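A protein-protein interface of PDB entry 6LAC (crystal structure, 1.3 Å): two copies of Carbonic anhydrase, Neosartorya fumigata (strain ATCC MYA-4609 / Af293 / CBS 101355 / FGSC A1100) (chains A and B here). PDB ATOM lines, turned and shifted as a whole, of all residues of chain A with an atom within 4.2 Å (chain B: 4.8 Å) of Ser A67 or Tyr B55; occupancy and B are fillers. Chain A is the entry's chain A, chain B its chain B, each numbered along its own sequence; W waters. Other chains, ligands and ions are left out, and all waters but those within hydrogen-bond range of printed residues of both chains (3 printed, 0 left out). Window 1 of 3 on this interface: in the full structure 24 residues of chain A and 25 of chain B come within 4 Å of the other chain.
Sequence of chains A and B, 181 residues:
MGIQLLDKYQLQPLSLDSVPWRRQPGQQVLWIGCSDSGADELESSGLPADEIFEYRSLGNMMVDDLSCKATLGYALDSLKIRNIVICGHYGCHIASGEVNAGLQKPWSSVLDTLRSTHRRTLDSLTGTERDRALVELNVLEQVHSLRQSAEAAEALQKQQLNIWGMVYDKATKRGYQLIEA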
ATOM      1  N   TYR A  55      -7.443  11.228  28.477  1.00  0.00           N
ATOM      2  CA  TYR A  55      -8.698  11.791  27.966  1.00  0.00           C
ATOM      3  C   TYR A  55      -8.322  12.495  26.686  1.00  0.00           C
ATOM      4  O   TYR A  55      -7.525  13.446  26.684  1.00  0.00           O
ATOM      5  CB  TYR A  55      -9.338  12.764  28.974  1.00  0.00           C
ATOM      6  CG  TYR A  55     -10.669  13.300  28.495  1.00  0.00           C
ATOM      7  CD1 TYR A  55     -11.712  12.411  28.235  1.00  0.00           C
ATOM      8  CD2 TYR A  55     -10.880  14.625  28.200  1.00  0.00           C
ATOM      9  CE1 TYR A  55     -12.934  12.814  27.715  1.00  0.00           C
ATOM     10  CE2 TYR A  55     -12.109  15.045  27.686  1.00  0.00           C
ATOM     11  CZ  TYR A  55     -13.120  14.135  27.426  1.00  0.00           C
ATOM     12  OH  TYR A  55     -14.322  14.445  26.814  1.00  0.00           O
ATOM     13  N   ARG A  56      -8.830  12.005  25.562  1.00  0.00           N
ATOM     14  CA  ARG A  56      -8.449  12.555  24.241  1.00  0.00           C
ATOM     15  C   ARG A  56      -9.681  13.070  23.558  1.00  0.00           C
ATOM     16  O   ARG A  56     -10.618  12.300  23.314  1.00  0.00           O
ATOM     17  CB  ARG A  56      -7.651  11.559  23.429  1.00  0.00           C
ATOM     18  CG  ARG A  56      -7.069  12.209  22.179  1.00  0.00           C
ATOM     19  CD  ARG A  56      -5.970  11.338  21.616  1.00  0.00           C
ATOM     20  NE  ARG A  56      -4.796  11.205  22.478  1.00  0.00           N
ATOM     21  CZ  ARG A  56      -3.761  12.030  22.552  1.00  0.00           C
ATOM     22  NH1 ARG A  56      -3.685  13.106  21.810  1.00  0.00           N
ATOM     23  NH2 ARG A  56      -2.814  11.764  23.442  1.00  0.00           N
ATOM     24  N   ASP A  65     -19.129  20.544  30.199  1.00  0.00           N
ATOM     25  CA  ASP A  65     -19.979  19.425  29.737  1.00  0.00           C
ATOM     26  C   ASP A  65     -19.831  18.269  30.719  1.00  0.00           C
ATOM     27  O   ASP A  65     -18.913  18.297  31.589  1.00  0.00           O
ATOM     28  CB  ASP A  65     -19.676  19.154  28.265  1.00  0.00           C
ATOM     29  CG  ASP A  65     -20.414  18.006  27.615  1.00  0.00           C
ATOM     30  OD1 ASP A  65     -21.673  18.014  27.693  1.00  0.00           O
ATOM     31  OD2 ASP A  65     -19.725  17.131  27.005  1.00  0.00           O
ATOM     32  N   LEU A  66     -20.751  17.320  30.662  1.00  0.00           N
ATOM     33  CA  LEU A  66     -20.747  16.175  31.587  1.00  0.00           C
ATOM     34  C   LEU A  66     -19.420  15.424  31.446  1.00  0.00           C
ATOM     35  O   LEU A  66     -18.888  15.020  32.502  1.00  0.00           O
ATOM     36  CB  LEU A  66     -21.917  15.247  31.249  1.00  0.00           C
ATOM     37  CG  LEU A  66     -23.323  15.835  31.384  1.00  0.00           C
ATOM     38  CD1 LEU A  66     -24.344  14.711  31.391  1.00  0.00           C
ATOM     39  CD2 LEU A  66     -23.432  16.680  32.644  1.00  0.00           C
ATOM     40  N   SER A  67     -18.968  15.169  30.221  1.00  0.00           N
ATOM     41  CA  SER A  67     -17.772  14.318  30.000  1.00  0.00           C
ATOM     42  C   SER A  67     -16.558  14.948  30.676  1.00  0.00           C
ATOM     43  O   SER A  67     -15.775  14.264  31.395  1.00  0.00           O
ATOM     44  CB  SER A  67     -17.492  14.101  28.540  1.00  0.00           C
ATOM     45  OG  SER A  67     -18.355  13.135  27.996  1.00  0.00           O
ATOM     46  N   CYS A  68     -16.403  16.231  30.489  1.00  0.00           N
ATOM     47  CA  CYS A  68     -15.168  16.877  30.959  1.00  0.00           C
ATOM     48  C   CYS A  68     -15.231  16.904  32.487  1.00  0.00           C
ATOM     49  O   CYS A  68     -14.266  16.512  33.127  1.00  0.00           O
ATOM     50  CB  CYS A  68     -14.999  18.240  30.311  1.00  0.00           C
ATOM     51  SG  CYS A  68     -14.789  18.204  28.511  1.00  0.00           S
ATOM     52  N   LYS A  69     -16.382  17.179  33.081  1.00  0.00           N
ATOM     53  CA  LYS A  69     -16.590  17.205  34.542  1.00  0.00           C
ATOM     54  C   LYS A  69     -16.445  15.814  35.184  1.00  0.00           C
ATOM     55  O   LYS A  69     -15.796  15.702  36.226  1.00  0.00           O
ATOM     56  CB  LYS A  69     -17.954  17.821  34.866  1.00  0.00           C
ATOM     57  CG  LYS A  69     -18.043  19.286  34.496  1.00  0.00           C
ATOM     58  CD  LYS A  69     -19.360  19.926  34.851  1.00  0.00           C
ATOM     59  CE  LYS A  69     -19.427  21.352  34.354  1.00  0.00           C
ATOM     60  NZ  LYS A  69     -18.541  22.240  35.145  1.00  0.00           N
ATOM     61  N   ALA A  70     -17.077  14.770  34.639  1.00  0.00           N
ATOM     62  CA  ALA A  70     -16.987  13.400  35.180  1.00  0.00           C
ATOM     63  C   ALA A  70     -15.555  12.853  35.061  1.00  0.00           C
ATOM     64  O   ALA A  70     -15.148  11.998  35.854  1.00  0.00           O
ATOM     65  CB  ALA A  70     -17.960  12.450  34.509  1.00  0.00           C
ATOM     66  N   THR A  71     -14.865  13.184  33.962  1.00  0.00           N
ATOM     67  CA  THR A  71     -13.501  12.657  33.745  1.00  0.00           C
ATOM     68  C   THR A  71     -12.573  13.264  34.806  1.00  0.00           C
ATOM     69  O   THR A  71     -11.810  12.541  35.460  1.00  0.00           O
ATOM     70  CB  THR A  71     -13.035  12.926  32.316  1.00  0.00           C
ATOM     71  OG1 THR A  71     -13.974  12.321  31.435  1.00  0.00           O
ATOM     72  CG2 THR A  71     -11.672  12.326  32.090  1.00  0.00           C
ATOM     73  N   LEU B  30     -12.699   6.937  13.285  1.00  0.00           N
ATOM     74  CA  LEU B  30     -12.950   7.400  14.664  1.00  0.00           C
ATOM     75  C   LEU B  30     -12.802   6.207  15.593  1.00  0.00           C
ATOM     76  O   LEU B  30     -13.539   5.203  15.439  1.00  0.00           O
ATOM     77  CB  LEU B  30     -14.354   7.999  14.757  1.00  0.00           C
ATOM     78  CG  LEU B  30     -14.889   8.257  16.157  1.00  0.00           C
ATOM     79  CD1 LEU B  30     -13.993   9.221  16.970  1.00  0.00           C
ATOM     80  CD2 LEU B  30     -16.308   8.841  16.090  1.00  0.00           C
ATOM     81  N   TRP B  31     -11.789   6.232  16.454  1.00  0.00           N
ATOM     82  CA  TRP B  31     -11.451   5.152  17.385  1.00  0.00           C
ATOM     83  C   TRP B  31     -11.893   5.623  18.741  1.00  0.00           C
ATOM     84  O   TRP B  31     -11.299   6.602  19.258  1.00  0.00           O
ATOM     85  CB  TRP B  31      -9.953   4.941  17.330  1.00  0.00           C
ATOM     86  CG  TRP B  31      -9.510   3.726  18.064  1.00  0.00           C
ATOM     87  CD1 TRP B  31      -9.270   3.582  19.401  1.00  0.00           C
ATOM     88  CD2 TRP B  31      -9.383   2.415  17.535  1.00  0.00           C
ATOM     89  NE1 TRP B  31      -8.958   2.291  19.702  1.00  0.00           N
ATOM     90  CE2 TRP B  31      -8.999   1.540  18.566  1.00  0.00           C
ATOM     91  CE3 TRP B  31      -9.494   1.912  16.242  1.00  0.00           C
ATOM     92  CZ2 TRP B  31      -8.754   0.183  18.332  1.00  0.00           C
ATOM     93  CZ3 TRP B  31      -9.303   0.568  16.025  1.00  0.00           C
ATOM     94  CH2 TRP B  31      -8.951  -0.282  17.047  1.00  0.00           C
ATOM     95  N   ILE B  32     -12.822   4.933  19.349  1.00  0.00           N
ATOM     96  CA  ILE B  32     -13.380   5.264  20.681  1.00  0.00           C
ATOM     97  C   ILE B  32     -12.813   4.253  21.660  1.00  0.00           C
ATOM     98  O   ILE B  32     -13.140   3.050  21.550  1.00  0.00           O
ATOM     99  CB  ILE B  32     -14.898   5.272  20.659  1.00  0.00           C
ATOM    100  CG1 ILE B  32     -15.424   6.366  19.735  1.00  0.00           C
ATOM    101  CG2 ILE B  32     -15.432   5.434  22.089  1.00  0.00           C
ATOM    102  CD1 ILE B  32     -16.857   6.186  19.300  1.00  0.00           C
ATOM    103  N   GLY B  33     -11.927   4.657  22.558  1.00  0.00           N
ATOM    104  CA  GLY B  33     -11.288   3.760  23.532  1.00  0.00           C
ATOM    105  C   GLY B  33     -11.448   4.329  24.913  1.00  0.00           C
ATOM    106  O   GLY B  33     -12.056   5.361  25.123  1.00  0.00           O
ATOM    107  N   PHE B  53      -8.403   8.959  14.414  1.00  0.00           N
ATOM    108  CA  PHE B  53      -9.025  10.135  15.045  1.00  0.00           C
ATOM    109  C   PHE B  53      -9.586   9.592  16.349  1.00  0.00           C
ATOM    110  O   PHE B  53     -10.534   8.826  16.335  1.00  0.00           O
ATOM    111  CB  PHE B  53     -10.068  10.748  14.129  1.00  0.00           C
ATOM    112  CG  PHE B  53     -10.674  11.984  14.702  1.00  0.00           C
ATOM    113  CD1 PHE B  53      -9.989  13.177  14.680  1.00  0.00           C
ATOM    114  CD2 PHE B  53     -11.941  11.971  15.224  1.00  0.00           C
ATOM    115  CE1 PHE B  53     -10.545  14.319  15.213  1.00  0.00           C
ATOM    116  CE2 PHE B  53     -12.497  13.096  15.778  1.00  0.00           C
ATOM    117  CZ  PHE B  53     -11.805  14.278  15.731  1.00  0.00           C
ATOM    118  N   GLU B  54      -8.887   9.885  17.451  1.00  0.00           N
ATOM    119  CA  GLU B  54      -9.065   9.109  18.691  1.00  0.00           C
ATOM    120  C   GLU B  54      -9.912   9.859  19.685  1.00  0.00           C
ATOM    121  O   GLU B  54      -9.518  11.003  20.086  1.00  0.00           O
ATOM    122  CB  GLU B  54      -7.680   8.847  19.268  1.00  0.00           C
ATOM    123  CG  GLU B  54      -7.639   7.934  20.472  1.00  0.00           C
ATOM    124  CD  GLU B  54      -6.247   7.588  20.978  1.00  0.00           C
ATOM    125  OE1 GLU B  54      -5.273   8.228  20.565  1.00  0.00           O
ATOM    126  OE2 GLU B  54      -6.151   6.680  21.838  1.00  0.00           O
ATOM    127  N   TYR B  55     -10.964   9.250  20.200  1.00  0.00           N
ATOM    128  CA  TYR B  55     -11.755   9.805  21.323  1.00  0.00           C
ATOM    129  C   TYR B  55     -11.639   8.825  22.441  1.00  0.00           C
ATOM    130  O   TYR B  55     -11.957   7.647  22.294  1.00  0.00           O
ATOM    131  CB  TYR B  55     -13.230   9.957  20.927  1.00  0.00           C
ATOM    132  CG  TYR B  55     -14.018  10.632  22.009  1.00  0.00           C
ATOM    133  CD1 TYR B  55     -13.715  11.940  22.402  1.00  0.00           C
ATOM    134  CD2 TYR B  55     -14.948   9.937  22.753  1.00  0.00           C
ATOM    135  CE1 TYR B  55     -14.330  12.534  23.505  1.00  0.00           C
ATOM    136  CE2 TYR B  55     -15.645  10.551  23.796  1.00  0.00           C
ATOM    137  CZ  TYR B  55     -15.289  11.826  24.207  1.00  0.00           C
ATOM    138  OH  TYR B  55     -15.925  12.431  25.278  1.00  0.00           O
ATOM    139  N   ARG B  56     -10.963   9.237  23.496  1.00  0.00           N
ATOM    140  CA  ARG B  56     -10.672   8.310  24.622  1.00  0.00           C
ATOM    141  C   ARG B  56     -11.328   8.861  25.877  1.00  0.00           C
ATOM    142  O   ARG B  56     -11.000   9.960  26.299  1.00  0.00           O
ATOM    143  CB  ARG B  56      -9.185   8.054  24.739  1.00  0.00           C
ATOM    144  CG  ARG B  56      -8.868   6.926  25.713  1.00  0.00           C
ATOM    145  CD  ARG B  56      -7.460   6.417  25.589  1.00  0.00           C
ATOM    146  NE  ARG B  56      -7.161   5.801  24.305  1.00  0.00           N
ATOM    147  CZ  ARG B  56      -7.421   4.546  23.956  1.00  0.00           C
ATOM    148  NH1 ARG B  56      -7.888   3.686  24.819  1.00  0.00           N
ATOM    149  NH2 ARG B  56      -7.181   4.130  22.724  1.00  0.00           N
ATOM    150  N   SER B  57     -12.211   8.045  26.432  1.00  0.00           N
ATOM    151  CA  SER B  57     -13.249   8.459  27.389  1.00  0.00           C
ATOM    152  C   SER B  57     -13.372   7.446  28.507  1.00  0.00           C
ATOM    153  O   SER B  57     -12.951   6.324  28.383  1.00  0.00           O
ATOM    154  CB  SER B  57     -14.603   8.556  26.623  1.00  0.00           C
ATOM    155  OG  SER B  57     -14.997   7.252  26.116  1.00  0.00           O
ATOM    156  N   MET B  61     -17.185   4.697  26.385  1.00  0.00           N
ATOM    157  CA  MET B  61     -18.622   4.978  26.198  1.00  0.00           C
ATOM    158  C   MET B  61     -18.863   6.274  25.455  1.00  0.00           C
ATOM    159  O   MET B  61     -18.032   7.181  25.507  1.00  0.00           O
ATOM    160  CB  MET B  61     -19.336   5.072  27.549  1.00  0.00           C
ATOM    161  CG  MET B  61     -19.229   3.818  28.327  1.00  0.00           C
ATOM    162  SD  MET B  61     -20.294   4.092  29.759  1.00  0.00           S
ATOM    163  CE  MET B  61     -19.800   2.664  30.672  1.00  0.00           C
ATOM    164  N   MET B  62     -19.951   6.322  24.705  1.00  0.00           N
ATOM    165  CA  MET B  62     -20.549   7.564  24.165  1.00  0.00           C
ATOM    166  C   MET B  62     -21.876   7.773  24.870  1.00  0.00           C
ATOM    167  O   MET B  62     -22.781   6.927  24.745  1.00  0.00           O
ATOM    168  CB  MET B  62     -20.744   7.434  22.648  1.00  0.00           C
ATOM    169  CG  MET B  62     -19.424   7.200  21.881  1.00  0.00           C
ATOM    170  SD  MET B  62     -18.330   8.614  21.929  1.00  0.00           S
ATOM    171  CE  MET B  62     -18.875   9.408  20.415  1.00  0.00           C
ATOM    172  N   VAL B  63     -21.936   8.763  25.726  1.00  0.00           N
ATOM    173  CA  VAL B  63     -23.163   9.019  26.499  1.00  0.00           C
ATOM    174  C   VAL B  63     -23.841  10.195  25.825  1.00  0.00           C
ATOM    175  O   VAL B  63     -23.291  10.764  24.847  1.00  0.00           O
ATOM    176  CB  VAL B  63     -22.781   9.201  27.972  1.00  0.00           C
ATOM    177  CG1 VAL B  63     -22.048   8.004  28.507  1.00  0.00           C
ATOM    178  CG2 VAL B  63     -21.970  10.464  28.189  1.00  0.00           C
ATOM    179  N   ASP B  65     -24.128  13.373  25.610  1.00  0.00           N
ATOM    180  CA  ASP B  65     -23.708  14.702  26.112  1.00  0.00           C
ATOM    181  C   ASP B  65     -23.129  15.520  24.975  1.00  0.00           C
ATOM    182  O   ASP B  65     -23.144  15.084  23.817  1.00  0.00           O
ATOM    183  CB  ASP B  65     -22.761  14.596  27.305  1.00  0.00           C
ATOM    184  CG  ASP B  65     -21.381  14.084  26.962  1.00  0.00           C
ATOM    185  OD1 ASP B  65     -21.148  13.640  25.807  1.00  0.00           O
ATOM    186  OD2 ASP B  65     -20.542  14.164  27.875  1.00  0.00           O
ATOM    187  N   SER B  67     -20.100  16.459  24.373  1.00  0.00           N
ATOM    188  CA  SER B  67     -18.811  15.896  23.877  1.00  0.00           C
ATOM    189  C   SER B  67     -19.061  14.773  22.865  1.00  0.00           C
ATOM    190  O   SER B  67     -18.456  14.753  21.799  1.00  0.00           O
ATOM    191  CB  SER B  67     -17.949  15.446  25.015  1.00  0.00           C
ATOM    192  OG  SER B  67     -17.421  16.549  25.690  1.00  0.00           O
ATOM    193  N   THR B  71     -18.133  15.368  18.932  1.00  0.00           N
ATOM    194  CA  THR B  71     -17.040  14.517  18.396  1.00  0.00           C
ATOM    195  C   THR B  71     -17.585  13.711  17.213  1.00  0.00           C
ATOM    196  O   THR B  71     -16.966  13.647  16.201  1.00  0.00           O
ATOM    197  CB  THR B  71     -16.456  13.667  19.529  1.00  0.00           C
ATOM    198  OG1 THR B  71     -15.987  14.517  20.581  1.00  0.00           O
ATOM    199  CG2 THR B  71     -15.355  12.783  18.995  1.00  0.00           C
ATOM    200  N   TRP B 107     -22.479   7.468  33.208  1.00  0.00           N
ATOM    201  CA  TRP B 107     -21.591   6.298  33.054  1.00  0.00           C
ATOM    202  C   TRP B 107     -21.979   5.201  34.037  1.00  0.00           C
ATOM    203  O   TRP B 107     -22.079   4.048  33.656  1.00  0.00           O
ATOM    204  CB  TRP B 107     -20.123   6.692  33.237  1.00  0.00           C
ATOM    205  CG  TRP B 107     -19.671   7.643  32.172  1.00  0.00           C
ATOM    206  CD1 TRP B 107     -19.063   7.296  30.985  1.00  0.00           C
ATOM    207  CD2 TRP B 107     -19.817   9.076  32.156  1.00  0.00           C
ATOM    208  NE1 TRP B 107     -18.849   8.423  30.266  1.00  0.00           N
ATOM    209  CE2 TRP B 107     -19.326   9.526  30.918  1.00  0.00           C
ATOM    210  CE3 TRP B 107     -20.374  10.011  33.026  1.00  0.00           C
ATOM    211  CZ2 TRP B 107     -19.322  10.853  30.567  1.00  0.00           C
ATOM    212  CZ3 TRP B 107     -20.433  11.320  32.637  1.00  0.00           C
ATOM    213  CH2 TRP B 107     -19.920  11.741  31.426  1.00  0.00           C
HETATM  214  O   HOH W   1     -14.783  16.510  25.202  1.00  0.00           O
HETATM  215  O   HOH W   2     -16.841  11.319  27.376  1.00  0.00           O
HETATM  216  O   HOH W   3      -2.913   8.502  21.937  1.00  0.00           O
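OG of Ser A67 sits at hydrogen-bond distance from OD2 of Asp B65, 2.4 Å away. NE of Arg A56 is in salt-bridge range of OE1 of Glu B54 (3.6 Å). The side-chain hydroxyl (OG) of Ser B67 sits at hydrogen-bond distance from the side-chain carboxylate (OD2) of Asp A65. The side-chain carboxylate (OD2) of Asp A65 lies close to the side-chain carboxylate (OD2) of Asp B65, 3.2 Å away. OH of Tyr B55 is in hydrogen-bond range of OH of Tyr A55. The backbone NH of Arg A56 sits at hydrogen-bond distance from the backbone carbonyl oxygen of Arg B56, at 3.1 Å.
O of Tyr B55 is in hydrogen-bond range of N of Gly B33 (3.0 Å). OG1 of Thr B71 is in hydrogen-bond range of O of Ser B67 (2.8 Å). The backbone carbonyl oxygen of Trp B31 is in hydrogen-bond range of the backbone NH of Tyr B55, 2.8 Å away. O of Ser A67 lies within hydrogen-bond range of OG1 of Thr A71 (2.6 Å). N of Ser B67 sits close to OD1 of Asp B65 (3.3 Å). OE2 of Glu B54 lies within salt-bridge range of NE of Arg B56.
Arg B56 touches Tyr A55 (O to CD1, 3.2 Å). Tyr A55 touches Ser B67. Arg A56 touches Tyr B55 (O to CD1, 3.2 Å). Leu A66 touches Asp B65 (CB to OD2, 3.8 Å). Leu A66 touches Trp B107 (O to CH2, 3.6 Å). Ser A67 touches Tyr B55. CB of Ser A67 touches OG of Ser B67 (3.8 Å). Ser A67 touches Trp B107 (OG to CZ2, 3.6 Å). Ala A70 touches Trp B107.
Of the printed residues of chain B, Ser A67 touches Tyr B55 (3.7 Å), Asp B65 (2.4 Å), Ser B67 (3.8 Å) and Trp B107 (3.6 Å). Of the printed residues of chain B, Leu A66 touches Asp B65 and Trp B107. Of the printed residues of chain B, Asp A65 touches Asp B65 (3.2 Å) and Ser B67 (2.7 Å). Printed residues of chain A within 4 Å of Glu B54: Arg A56. Printed residues of chain B within 4 Å of Tyr A55: Tyr B55 (3.0 Å), Arg B56 (3.2 Å) and Ser B67 (3.9 Å). Of the printed residues of chain A, Asp B65 touches Asp A65, Leu A66 and Ser A67. The nearest residue of chain B that does not touch Ser A67 is Val B63 (4.5 Å).
Printed residues of chain B that touch a printed residue of chain A: Glu B54, Tyr B55, Arg B56, Asp B65, Ser B67 and Trp B107. Of the 9 printed residues of chain A, 6 touch a printed residue of chain B. Along chain A the printed residues that touch a printed residue of chain B span positions 55 to 70.
Tyr A55 touches Arg B56, and with the chains exchanged Arg A56 touches Tyr B55. Tyr A55 touches Ser B67, and with the chains exchanged Ser A67 touches Tyr B55. Arg B56 touches its own counterpart, Arg A56. Asp A65 touches Ser B67, and with the chains exchanged Ser A67 touches Asp B65. 5 positions are printed for both chains.
Water W2 lies within hydrogen-bond range of the side-chain hydroxyl of Ser A67 (2.4 Å) and the side-chain hydroxyl of Tyr B55 (2.5 Å). Water W1 lies within hydrogen-bond range of OH of Tyr A55 (2.7 Å), OG of Ser B67 (2.7 Å) and SG of Cys A68 (3.7 Å). Water W3 lies within hydrogen-bond range of OE1 of Glu B54 (2.7 Å) and NE of Arg A56 (3.3 Å).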
